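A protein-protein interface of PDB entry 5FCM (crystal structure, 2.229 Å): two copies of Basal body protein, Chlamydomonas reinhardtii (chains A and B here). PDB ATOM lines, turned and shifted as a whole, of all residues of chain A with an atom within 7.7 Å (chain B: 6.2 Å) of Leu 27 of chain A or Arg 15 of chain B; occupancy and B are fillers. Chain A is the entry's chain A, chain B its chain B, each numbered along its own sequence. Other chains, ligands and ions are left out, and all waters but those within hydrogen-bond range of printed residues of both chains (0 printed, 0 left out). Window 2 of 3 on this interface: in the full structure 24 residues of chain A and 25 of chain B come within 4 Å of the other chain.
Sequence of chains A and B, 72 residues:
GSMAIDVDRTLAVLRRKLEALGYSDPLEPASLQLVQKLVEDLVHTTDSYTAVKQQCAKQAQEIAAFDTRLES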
ATOM      1  N   TYR A  23      29.487  -6.589   0.267  1.00  0.00           N
ATOM      2  CA  TYR A  23      28.503  -6.256   1.294  1.00  0.00           C
ATOM      3  C   TYR A  23      28.644  -4.798   1.725  1.00  0.00           C
ATOM      4  O   TYR A  23      28.156  -4.401   2.783  1.00  0.00           O
ATOM      5  CB  TYR A  23      28.657  -7.180   2.504  1.00  0.00           C
ATOM      6  CG  TYR A  23      28.130  -8.580   2.280  1.00  0.00           C
ATOM      7  CD1 TYR A  23      28.906  -9.546   1.652  1.00  0.00           C
ATOM      8  CD2 TYR A  23      26.856  -8.936   2.700  1.00  0.00           C
ATOM      9  CE1 TYR A  23      28.426 -10.827   1.446  1.00  0.00           C
ATOM     10  CE2 TYR A  23      26.366 -10.213   2.500  1.00  0.00           C
ATOM     11  CZ  TYR A  23      27.154 -11.153   1.871  1.00  0.00           C
ATOM     12  OH  TYR A  23      26.670 -12.426   1.672  1.00  0.00           O
ATOM     13  N   SER A  24      29.313  -4.003   0.896  1.00  0.00           N
ATOM     14  CA  SER A  24      29.537  -2.595   1.198  1.00  0.00           C
ATOM     15  C   SER A  24      28.321  -1.754   0.823  1.00  0.00           C
ATOM     16  O   SER A  24      28.122  -0.663   1.358  1.00  0.00           O
ATOM     17  CB  SER A  24      30.777  -2.087   0.461  1.00  0.00           C
ATOM     18  OG  SER A  24      31.920  -2.848   0.811  1.00  0.00           O
ATOM     19  N   ASP A  25      27.510  -2.265  -0.097  1.00  0.00           N
ATOM     20  CA  ASP A  25      26.294  -1.580  -0.515  1.00  0.00           C
ATOM     21  C   ASP A  25      25.114  -2.039   0.346  1.00  0.00           C
ATOM     22  O   ASP A  25      24.602  -3.139   0.153  1.00  0.00           O
ATOM     23  CB  ASP A  25      26.014  -1.850  -1.995  1.00  0.00           C
ATOM     24  CG  ASP A  25      24.887  -0.997  -2.541  1.00  0.00           C
ATOM     25  OD1 ASP A  25      24.135  -0.411  -1.736  1.00  0.00           O
ATOM     26  OD2 ASP A  25      24.753  -0.914  -3.780  1.00  0.00           O
ATOM     27  N   PRO A  26      24.675  -1.197   1.301  1.00  0.00           N
ATOM     28  CA  PRO A  26      23.622  -1.640   2.225  1.00  0.00           C
ATOM     29  C   PRO A  26      22.278  -1.937   1.563  1.00  0.00           C
ATOM     30  O   PRO A  26      21.432  -2.580   2.188  1.00  0.00           O
ATOM     31  CB  PRO A  26      23.490  -0.463   3.200  1.00  0.00           C
ATOM     32  CG  PRO A  26      24.040   0.707   2.477  1.00  0.00           C
ATOM     33  CD  PRO A  26      25.128   0.172   1.605  1.00  0.00           C
ATOM     34  N   LEU A  27      22.078  -1.480   0.331  1.00  0.00           N
ATOM     35  CA  LEU A  27      20.824  -1.742  -0.373  1.00  0.00           C
ATOM     36  C   LEU A  27      20.937  -2.964  -1.283  1.00  0.00           C
ATOM     37  O   LEU A  27      19.977  -3.332  -1.960  1.00  0.00           O
ATOM     38  CB  LEU A  27      20.397  -0.518  -1.187  1.00  0.00           C
ATOM     39  CG  LEU A  27      20.054   0.745  -0.389  1.00  0.00           C
ATOM     40  CD1 LEU A  27      19.609   1.855  -1.331  1.00  0.00           C
ATOM     41  CD2 LEU A  27      18.979   0.483   0.661  1.00  0.00           C
ATOM     42  N   GLU A  28      22.111  -3.585  -1.304  1.00  0.00           N
ATOM     43  CA  GLU A  28      22.288  -4.863  -1.980  1.00  0.00           C
ATOM     44  C   GLU A  28      21.459  -5.904  -1.225  1.00  0.00           C
ATOM     45  O   GLU A  28      21.403  -5.869   0.003  1.00  0.00           O
ATOM     46  CB  GLU A  28      23.772  -5.247  -2.017  1.00  0.00           C
ATOM     47  CG  GLU A  28      24.272  -5.892  -3.307  1.00  0.00           C
ATOM     48  CD  GLU A  28      23.930  -5.089  -4.549  1.00  0.00           C
ATOM     49  OE1 GLU A  28      24.782  -4.290  -4.995  1.00  0.00           O
ATOM     50  OE2 GLU A  28      22.812  -5.260  -5.082  1.00  0.00           O
ATOM     51  N   PRO A  29      20.805  -6.830  -1.947  1.00  0.00           N
ATOM     52  CA  PRO A  29      19.901  -7.750  -1.246  1.00  0.00           C
ATOM     53  C   PRO A  29      20.604  -8.578  -0.176  1.00  0.00           C
ATOM     54  O   PRO A  29      20.017  -8.868   0.866  1.00  0.00           O
ATOM     55  CB  PRO A  29      19.374  -8.647  -2.369  1.00  0.00           C
ATOM     56  CG  PRO A  29      20.422  -8.587  -3.420  1.00  0.00           C
ATOM     57  CD  PRO A  29      20.948  -7.189  -3.369  1.00  0.00           C
ATOM     58  N   ALA A  30      21.852  -8.948  -0.436  1.00  0.00           N
ATOM     59  CA  ALA A  30      22.629  -9.729   0.515  1.00  0.00           C
ATOM     60  C   ALA A  30      22.843  -8.948   1.807  1.00  0.00           C
ATOM     61  O   ALA A  30      22.849  -9.520   2.896  1.00  0.00           O
ATOM     62  CB  ALA A  30      23.963 -10.126  -0.093  1.00  0.00           C
ATOM     63  N   SER A  31      23.020  -7.637   1.680  1.00  0.00           N
ATOM     64  CA  SER A  31      23.264  -6.789   2.839  1.00  0.00           C
ATOM     65  C   SER A  31      21.994  -6.613   3.664  1.00  0.00           C
ATOM     66  O   SER A  31      22.030  -6.679   4.892  1.00  0.00           O
ATOM     67  CB  SER A  31      23.804  -5.428   2.399  1.00  0.00           C
ATOM     68  OG  SER A  31      25.099  -5.560   1.838  1.00  0.00           O
ATOM     69  N   LEU A  32      20.872  -6.400   2.984  1.00  0.00           N
ATOM     70  CA  LEU A  32      19.597  -6.183   3.657  1.00  0.00           C
ATOM     71  C   LEU A  32      19.131  -7.434   4.397  1.00  0.00           C
ATOM     72  O   LEU A  32      18.504  -7.339   5.451  1.00  0.00           O
ATOM     73  CB  LEU A  32      18.532  -5.748   2.650  1.00  0.00           C
ATOM     74  CG  LEU A  32      18.705  -4.350   2.054  1.00  0.00           C
ATOM     75  CD1 LEU A  32      17.753  -4.152   0.888  1.00  0.00           C
ATOM     76  CD2 LEU A  32      18.481  -3.282   3.115  1.00  0.00           C
ATOM     77  N   ASP B   8      12.998   4.356  -1.867  1.00  0.00           N
ATOM     78  CA  ASP B   8      14.198   3.771  -2.454  1.00  0.00           C
ATOM     79  C   ASP B   8      14.838   4.724  -3.466  1.00  0.00           C
ATOM     80  O   ASP B   8      16.064   4.830  -3.544  1.00  0.00           O
ATOM     81  CB  ASP B   8      13.863   2.432  -3.117  1.00  0.00           C
ATOM     82  CG  ASP B   8      15.087   1.727  -3.669  1.00  0.00           C
ATOM     83  OD1 ASP B   8      16.184   1.890  -3.095  1.00  0.00           O
ATOM     84  OD2 ASP B   8      14.946   1.002  -4.677  1.00  0.00           O
ATOM     85  N   THR B  10      14.434   8.065  -3.546  1.00  0.00           N
ATOM     86  CA  THR B  10      14.886   9.275  -2.866  1.00  0.00           C
ATOM     87  C   THR B  10      16.316   9.092  -2.369  1.00  0.00           C
ATOM     88  O   THR B  10      17.134  10.009  -2.450  1.00  0.00           O
ATOM     89  CB  THR B  10      13.981   9.636  -1.675  1.00  0.00           C
ATOM     90  OG1 THR B  10      14.110   8.638  -0.654  1.00  0.00           O
ATOM     91  CG2 THR B  10      12.529   9.733  -2.110  1.00  0.00           C
ATOM     92  N   LEU B  11      16.611   7.901  -1.858  1.00  0.00           N
ATOM     93  CA  LEU B  11      17.937   7.590  -1.340  1.00  0.00           C
ATOM     94  C   LEU B  11      18.956   7.466  -2.467  1.00  0.00           C
ATOM     95  O   LEU B  11      20.110   7.864  -2.317  1.00  0.00           O
ATOM     96  CB  LEU B  11      17.907   6.294  -0.526  1.00  0.00           C
ATOM     97  CG  LEU B  11      16.945   6.263   0.664  1.00  0.00           C
ATOM     98  CD1 LEU B  11      16.965   4.895   1.331  1.00  0.00           C
ATOM     99  CD2 LEU B  11      17.273   7.354   1.673  1.00  0.00           C
ATOM    100  N   ALA B  12      18.526   6.904  -3.592  1.00  0.00           N
ATOM    101  CA  ALA B  12      19.409   6.733  -4.739  1.00  0.00           C
ATOM    102  C   ALA B  12      19.815   8.098  -5.290  1.00  0.00           C
ATOM    103  O   ALA B  12      20.990   8.343  -5.561  1.00  0.00           O
ATOM    104  CB  ALA B  12      18.733   5.899  -5.814  1.00  0.00           C
ATOM    105  N   VAL B  13      18.832   8.979  -5.446  1.00  0.00           N
ATOM    106  CA  VAL B  13      19.077  10.350  -5.883  1.00  0.00           C
ATOM    107  C   VAL B  13      20.049  11.018  -4.920  1.00  0.00           C
ATOM    108  O   VAL B  13      21.065  11.579  -5.335  1.00  0.00           O
ATOM    109  CB  VAL B  13      17.754  11.146  -5.980  1.00  0.00           C
ATOM    110  CG1 VAL B  13      18.011  12.653  -6.070  1.00  0.00           C
ATOM    111  CG2 VAL B  13      16.942  10.675  -7.172  1.00  0.00           C
ATOM    112  N   LEU B  14      19.730  10.946  -3.631  1.00  0.00           N
ATOM    113  CA  LEU B  14      20.547  11.566  -2.597  1.00  0.00           C
ATOM    114  C   LEU B  14      21.965  10.999  -2.608  1.00  0.00           C
ATOM    115  O   LEU B  14      22.935  11.721  -2.374  1.00  0.00           O
ATOM    116  CB  LEU B  14      19.905  11.368  -1.226  1.00  0.00           C
ATOM    117  CG  LEU B  14      20.574  12.088  -0.054  1.00  0.00           C
ATOM    118  CD1 LEU B  14      20.536  13.601  -0.242  1.00  0.00           C
ATOM    119  CD2 LEU B  14      19.904  11.695   1.248  1.00  0.00           C
ATOM    120  N   ARG B  15      22.079   9.704  -2.883  1.00  0.00           N
ATOM    121  CA  ARG B  15      23.382   9.060  -3.020  1.00  0.00           C
ATOM    122  C   ARG B  15      24.201   9.690  -4.144  1.00  0.00           C
ATOM    123  O   ARG B  15      25.378  10.000  -3.971  1.00  0.00           O
ATOM    124  CB  ARG B  15      23.214   7.566  -3.293  1.00  0.00           C
ATOM    125  CG  ARG B  15      22.994   6.713  -2.063  1.00  0.00           C
ATOM    126  CD  ARG B  15      22.660   5.285  -2.464  1.00  0.00           C
ATOM    127  NE  ARG B  15      23.323   4.300  -1.618  1.00  0.00           N
ATOM    128  CZ  ARG B  15      23.333   2.993  -1.858  1.00  0.00           C
ATOM    129  NH1 ARG B  15      22.717   2.504  -2.926  1.00  0.00           N
ATOM    130  NH2 ARG B  15      23.965   2.172  -1.031  1.00  0.00           N
ATOM    131  N   ARG B  16      23.570   9.864  -5.299  1.00  0.00           N
ATOM    132  CA  ARG B  16      24.250  10.379  -6.480  1.00  0.00           C
ATOM    133  C   ARG B  16      24.785  11.787  -6.235  1.00  0.00           C
ATOM    134  O   ARG B  16      25.955  12.071  -6.489  1.00  0.00           O
ATOM    135  CB  ARG B  16      23.298  10.373  -7.679  1.00  0.00           C
ATOM    136  CG  ARG B  16      23.930  10.800  -9.001  1.00  0.00           C
ATOM    137  CD  ARG B  16      23.435  12.166  -9.443  1.00  0.00           C
ATOM    138  NE  ARG B  16      21.979  12.215  -9.541  1.00  0.00           N
ATOM    139  CZ  ARG B  16      21.273  13.332  -9.691  1.00  0.00           C
ATOM    140  NH1 ARG B  16      21.886  14.506  -9.760  1.00  0.00           N
ATOM    141  NH2 ARG B  16      19.951  13.275  -9.767  1.00  0.00           N
ATOM    142  N   LYS B  17      23.922  12.660  -5.726  1.00  0.00           N
ATOM    143  CA  LYS B  17      24.288  14.050  -5.483  1.00  0.00           C
ATOM    144  C   LYS B  17      25.415  14.184  -4.461  1.00  0.00           C
ATOM    145  O   LYS B  17      26.160  15.163  -4.482  1.00  0.00           O
ATOM    146  CB  LYS B  17      23.064  14.838  -5.014  1.00  0.00           C
ATOM    147  CG  LYS B  17      22.003  14.992  -6.089  1.00  0.00           C
ATOM    148  CD  LYS B  17      20.847  15.859  -5.630  1.00  0.00           C
ATOM    149  CE  LYS B  17      19.920  16.188  -6.792  1.00  0.00           C
ATOM    150  NZ  LYS B  17      18.689  16.900  -6.352  1.00  0.00           N
ATOM    151  N   LEU B  18      25.539  13.204  -3.573  1.00  0.00           N
ATOM    152  CA  LEU B  18      26.577  13.231  -2.549  1.00  0.00           C
ATOM    153  C   LEU B  18      27.902  12.700  -3.087  1.00  0.00           C
ATOM    154  O   LEU B  18      28.972  13.126  -2.650  1.00  0.00           O
ATOM    155  CB  LEU B  18      26.140  12.423  -1.325  1.00  0.00           C
ATOM    156  CG  LEU B  18      25.201  13.171  -0.375  1.00  0.00           C
ATOM    157  CD1 LEU B  18      24.490  12.212   0.557  1.00  0.00           C
ATOM    158  CD2 LEU B  18      25.973  14.210   0.428  1.00  0.00           C
ATOM    159  N   GLU B  19      27.829  11.766  -4.028  1.00  0.00           N
ATOM    160  CA  GLU B  19      29.029  11.275  -4.696  1.00  0.00           C
ATOM    161  C   GLU B  19      29.667  12.399  -5.501  1.00  0.00           C
ATOM    162  O   GLU B  19      30.890  12.536  -5.542  1.00  0.00           O
ATOM    163  CB  GLU B  19      28.700  10.100  -5.613  1.00  0.00           C
ATOM    164  CG  GLU B  19      28.249   8.854  -4.891  1.00  0.00           C
ATOM    165  CD  GLU B  19      27.827   7.761  -5.851  1.00  0.00           C
ATOM    166  OE1 GLU B  19      27.512   6.645  -5.386  1.00  0.00           O
ATOM    167  OE2 GLU B  19      27.810   8.023  -7.073  1.00  0.00           O
ATOM    168  N   ALA B  20      28.823  13.200  -6.143  1.00  0.00           N
ATOM    169  CA  ALA B  20      29.285  14.327  -6.939  1.00  0.00           C
ATOM    170  C   ALA B  20      30.062  15.309  -6.071  1.00  0.00           C
ATOM    171  O   ALA B  20      31.060  15.888  -6.506  1.00  0.00           O
ATOM    172  CB  ALA B  20      28.107  15.020  -7.605  1.00  0.00           C
ATOM    173  N   TYR B  23      31.299  12.864  -1.343  1.00  0.00           N
ATOM    174  CA  TYR B  23      30.918  12.170  -0.111  1.00  0.00           C
ATOM    175  C   TYR B  23      30.591  10.700  -0.368  1.00  0.00           C
ATOM    176  O   TYR B  23      29.870  10.367  -1.308  1.00  0.00           O
ATOM    177  CB  TYR B  23      29.716  12.855   0.543  1.00  0.00           C
ATOM    178  CG  TYR B  23      30.045  14.186   1.180  1.00  0.00           C
ATOM    179  CD1 TYR B  23      30.506  14.254   2.487  1.00  0.00           C
ATOM    180  CD2 TYR B  23      29.897  15.372   0.475  1.00  0.00           C
ATOM    181  CE1 TYR B  23      30.811  15.466   3.076  1.00  0.00           C
ATOM    182  CE2 TYR B  23      30.199  16.590   1.055  1.00  0.00           C
ATOM    183  CZ  TYR B  23      30.656  16.630   2.357  1.00  0.00           C
ATOM    184  OH  TYR B  23      30.958  17.837   2.943  1.00  0.00           O
ATOM    185  N   ASP B  25      28.882   6.966   0.305  1.00  0.00           N
ATOM    186  CA  ASP B  25      27.502   6.560   0.552  1.00  0.00           C
ATOM    187  C   ASP B  25      27.090   6.831   2.004  1.00  0.00           C
ATOM    188  O   ASP B  25      27.712   6.308   2.927  1.00  0.00           O
ATOM    189  CB  ASP B  25      27.330   5.075   0.226  1.00  0.00           C
ATOM    190  CG  ASP B  25      25.932   4.573   0.511  1.00  0.00           C
ATOM    191  OD1 ASP B  25      24.987   5.390   0.483  1.00  0.00           O
ATOM    192  OD2 ASP B  25      25.776   3.359   0.759  1.00  0.00           O
ATOM    193  N   PRO B  26      26.045   7.654   2.212  1.00  0.00           N
ATOM    194  CA  PRO B  26      25.624   7.977   3.581  1.00  0.00           C
ATOM    195  C   PRO B  26      24.863   6.849   4.278  1.00  0.00           C
ATOM    196  O   PRO B  26      24.749   6.858   5.505  1.00  0.00           O
ATOM    197  CB  PRO B  26      24.713   9.190   3.383  1.00  0.00           C
ATOM    198  CG  PRO B  26      24.140   8.995   2.029  1.00  0.00           C
ATOM    199  CD  PRO B  26      25.244   8.383   1.211  1.00  0.00           C
ATOM    200  N   LEU B  27      24.352   5.897   3.506  1.00  0.00           N
ATOM    201  CA  LEU B  27      23.593   4.787   4.069  1.00  0.00           C
ATOM    202  C   LEU B  27      24.512   3.776   4.742  1.00  0.00           C
ATOM    203  O   LEU B  27      24.116   3.102   5.692  1.00  0.00           O
ATOM    204  CB  LEU B  27      22.771   4.092   2.983  1.00  0.00           C
ATOM    205  CG  LEU B  27      21.863   4.997   2.145  1.00  0.00           C
ATOM    206  CD1 LEU B  27      21.095   4.171   1.120  1.00  0.00           C
ATOM    207  CD2 LEU B  27      20.908   5.789   3.028  1.00  0.00           C
ATOM    208  N   GLU B  28      25.741   3.668   4.247  1.00  0.00           N
ATOM    209  CA  GLU B  28      26.675   2.681   4.776  1.00  0.00           C
ATOM    210  C   GLU B  28      26.986   2.960   6.254  1.00  0.00           C
ATOM    211  O   GLU B  28      26.841   2.068   7.087  1.00  0.00           O
ATOM    212  CB  GLU B  28      27.952   2.646   3.923  1.00  0.00           C
ATOM    213  CG  GLU B  28      29.116   1.857   4.511  1.00  0.00           C
ATOM    214  CD  GLU B  28      28.839   0.367   4.576  1.00  0.00           C
ATOM    215  OE1 GLU B  28      27.704  -0.045   4.254  1.00  0.00           O
ATOM    216  OE2 GLU B  28      29.760  -0.396   4.944  1.00  0.00           O
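OD1 of Asp 25 of chain A is in salt-bridge range of NH2 of Arg 15 of chain B (2.7 Å).
The side-chain carboxylate (OE1) of Glu 28 of chain B sits close to the backbone carbonyl oxygen (O) of Ser 24 of chain A (3.0 Å).
The side-chain carboxylate (OD1) of Asp 25 of chain A sits close to the backbone NH (N) of Leu 27 of chain A (3.1 Å).
The side-chain hydroxyl (OG) of Ser 31 of chain A sits at hydrogen-bond distance from the backbone carbonyl oxygen (O) of Asp 25 of chain A (3.0 Å).
The guanidinium group (NH2) of Arg 15 of chain B lies within salt-bridge range of the side-chain carboxylate (OD2) of Asp 25 of chain B.
OD1 of Asp 25 of chain B lies within hydrogen-bond range of N of Leu 27 of chain B, at 3.1 Å.
CD of Pro 26 of chain A touches NH2 of Arg 15 of chain B, at 3.5 Å.
Pro 26 of chain A touches Asp 25 of chain B (CD to OD2, 3.4 Å).
CB of Leu 27 of chain B touches CG of Pro 26 of chain A, 3.7 Å away.
Glu 28 of chain B touches Pro 26 of chain A.
CD1 of Leu 27 of chain A touches OD1 of Asp 8 of chain B, 3.9 Å away.
Leu 27 of chain A touches Arg 15 of chain B.
Leu 27 of chain A touches Leu 27 of chain B (CD1 to CD1, 3.7 Å).
Of chain B, only Asp 8 (3.9 Å), Arg 15 (3.6 Å) and Leu 27 (3.7 Å) come within 4 Å of Leu 27 of chain A.
Printed residues of chain A within 4 Å of Arg 15 of chain B: Asp 25 (2.7 Å), Pro 26 (3.5 Å) and Leu 27 (3.6 Å).
Printed residues of chain B within 4 Å of Pro 26 of chain A: Arg 15, Asp 25, Leu 27 and Glu 28.
Of the printed residues of chain A, Leu 27 of chain B touches Pro 26 (3.7 Å) and Leu 27 (3.7 Å).
Of the printed residues of chain B, Asp 25 of chain A touches Arg 15 (2.7 Å).
Printed residues of chain A within 4 Å of Glu 28 of chain B: Ser 24 (3.0 Å) and Pro 26 (3.7 Å).
Printed residues of chain B within 4 Å of Ser 24 of chain A: Glu 28.
Val 13 of chain B touches none of the printed residues of chain A.
Tyr 23 of chain A touches none of the printed residues of chain B.
The nearest residue of chain A that does not touch Arg 15 of chain B is Ser 24 of chain A (5.6 Å).
The nearest printed residue of chain B that does not touch Ser 24 of chain A is Asp 25 of chain B (4.7 Å).
Of the 10 printed residues of chain A, 4 touch a printed residue of chain B.
Of the 17 printed residues of chain B, 5 touch a printed residue of chain A.
Hydrophobic or aromatic side chains of chain B within 4 Å of the printed part of chain A: Leu 27.
Among the printed residues, 9 pairs touch across the chains.
Pro 26 of chain A touches Asp 25 of chain B, but with the chains exchanged Asp 25 of chain A does not touch Pro 26 of chain B (9.2 Å).
Pro 26 of chain A touches Leu 27 of chain B, but with the chains exchanged Leu 27 of chain A does not touch Pro 26 of chain B (9.0 Å).
Pro 26 of chain A touches Glu 28 of chain B, but with the chains exchanged Glu 28 of chain A does not touch Pro 26 of chain B (12.1 Å).
Leu 27 of chain B touches its own counterpart, Leu 27 of chain A.
5 positions are printed for both chains.
Of the 9 pairs that touch across the chains among the printed residues, 1 has its exchanged pair printed and touching as well.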
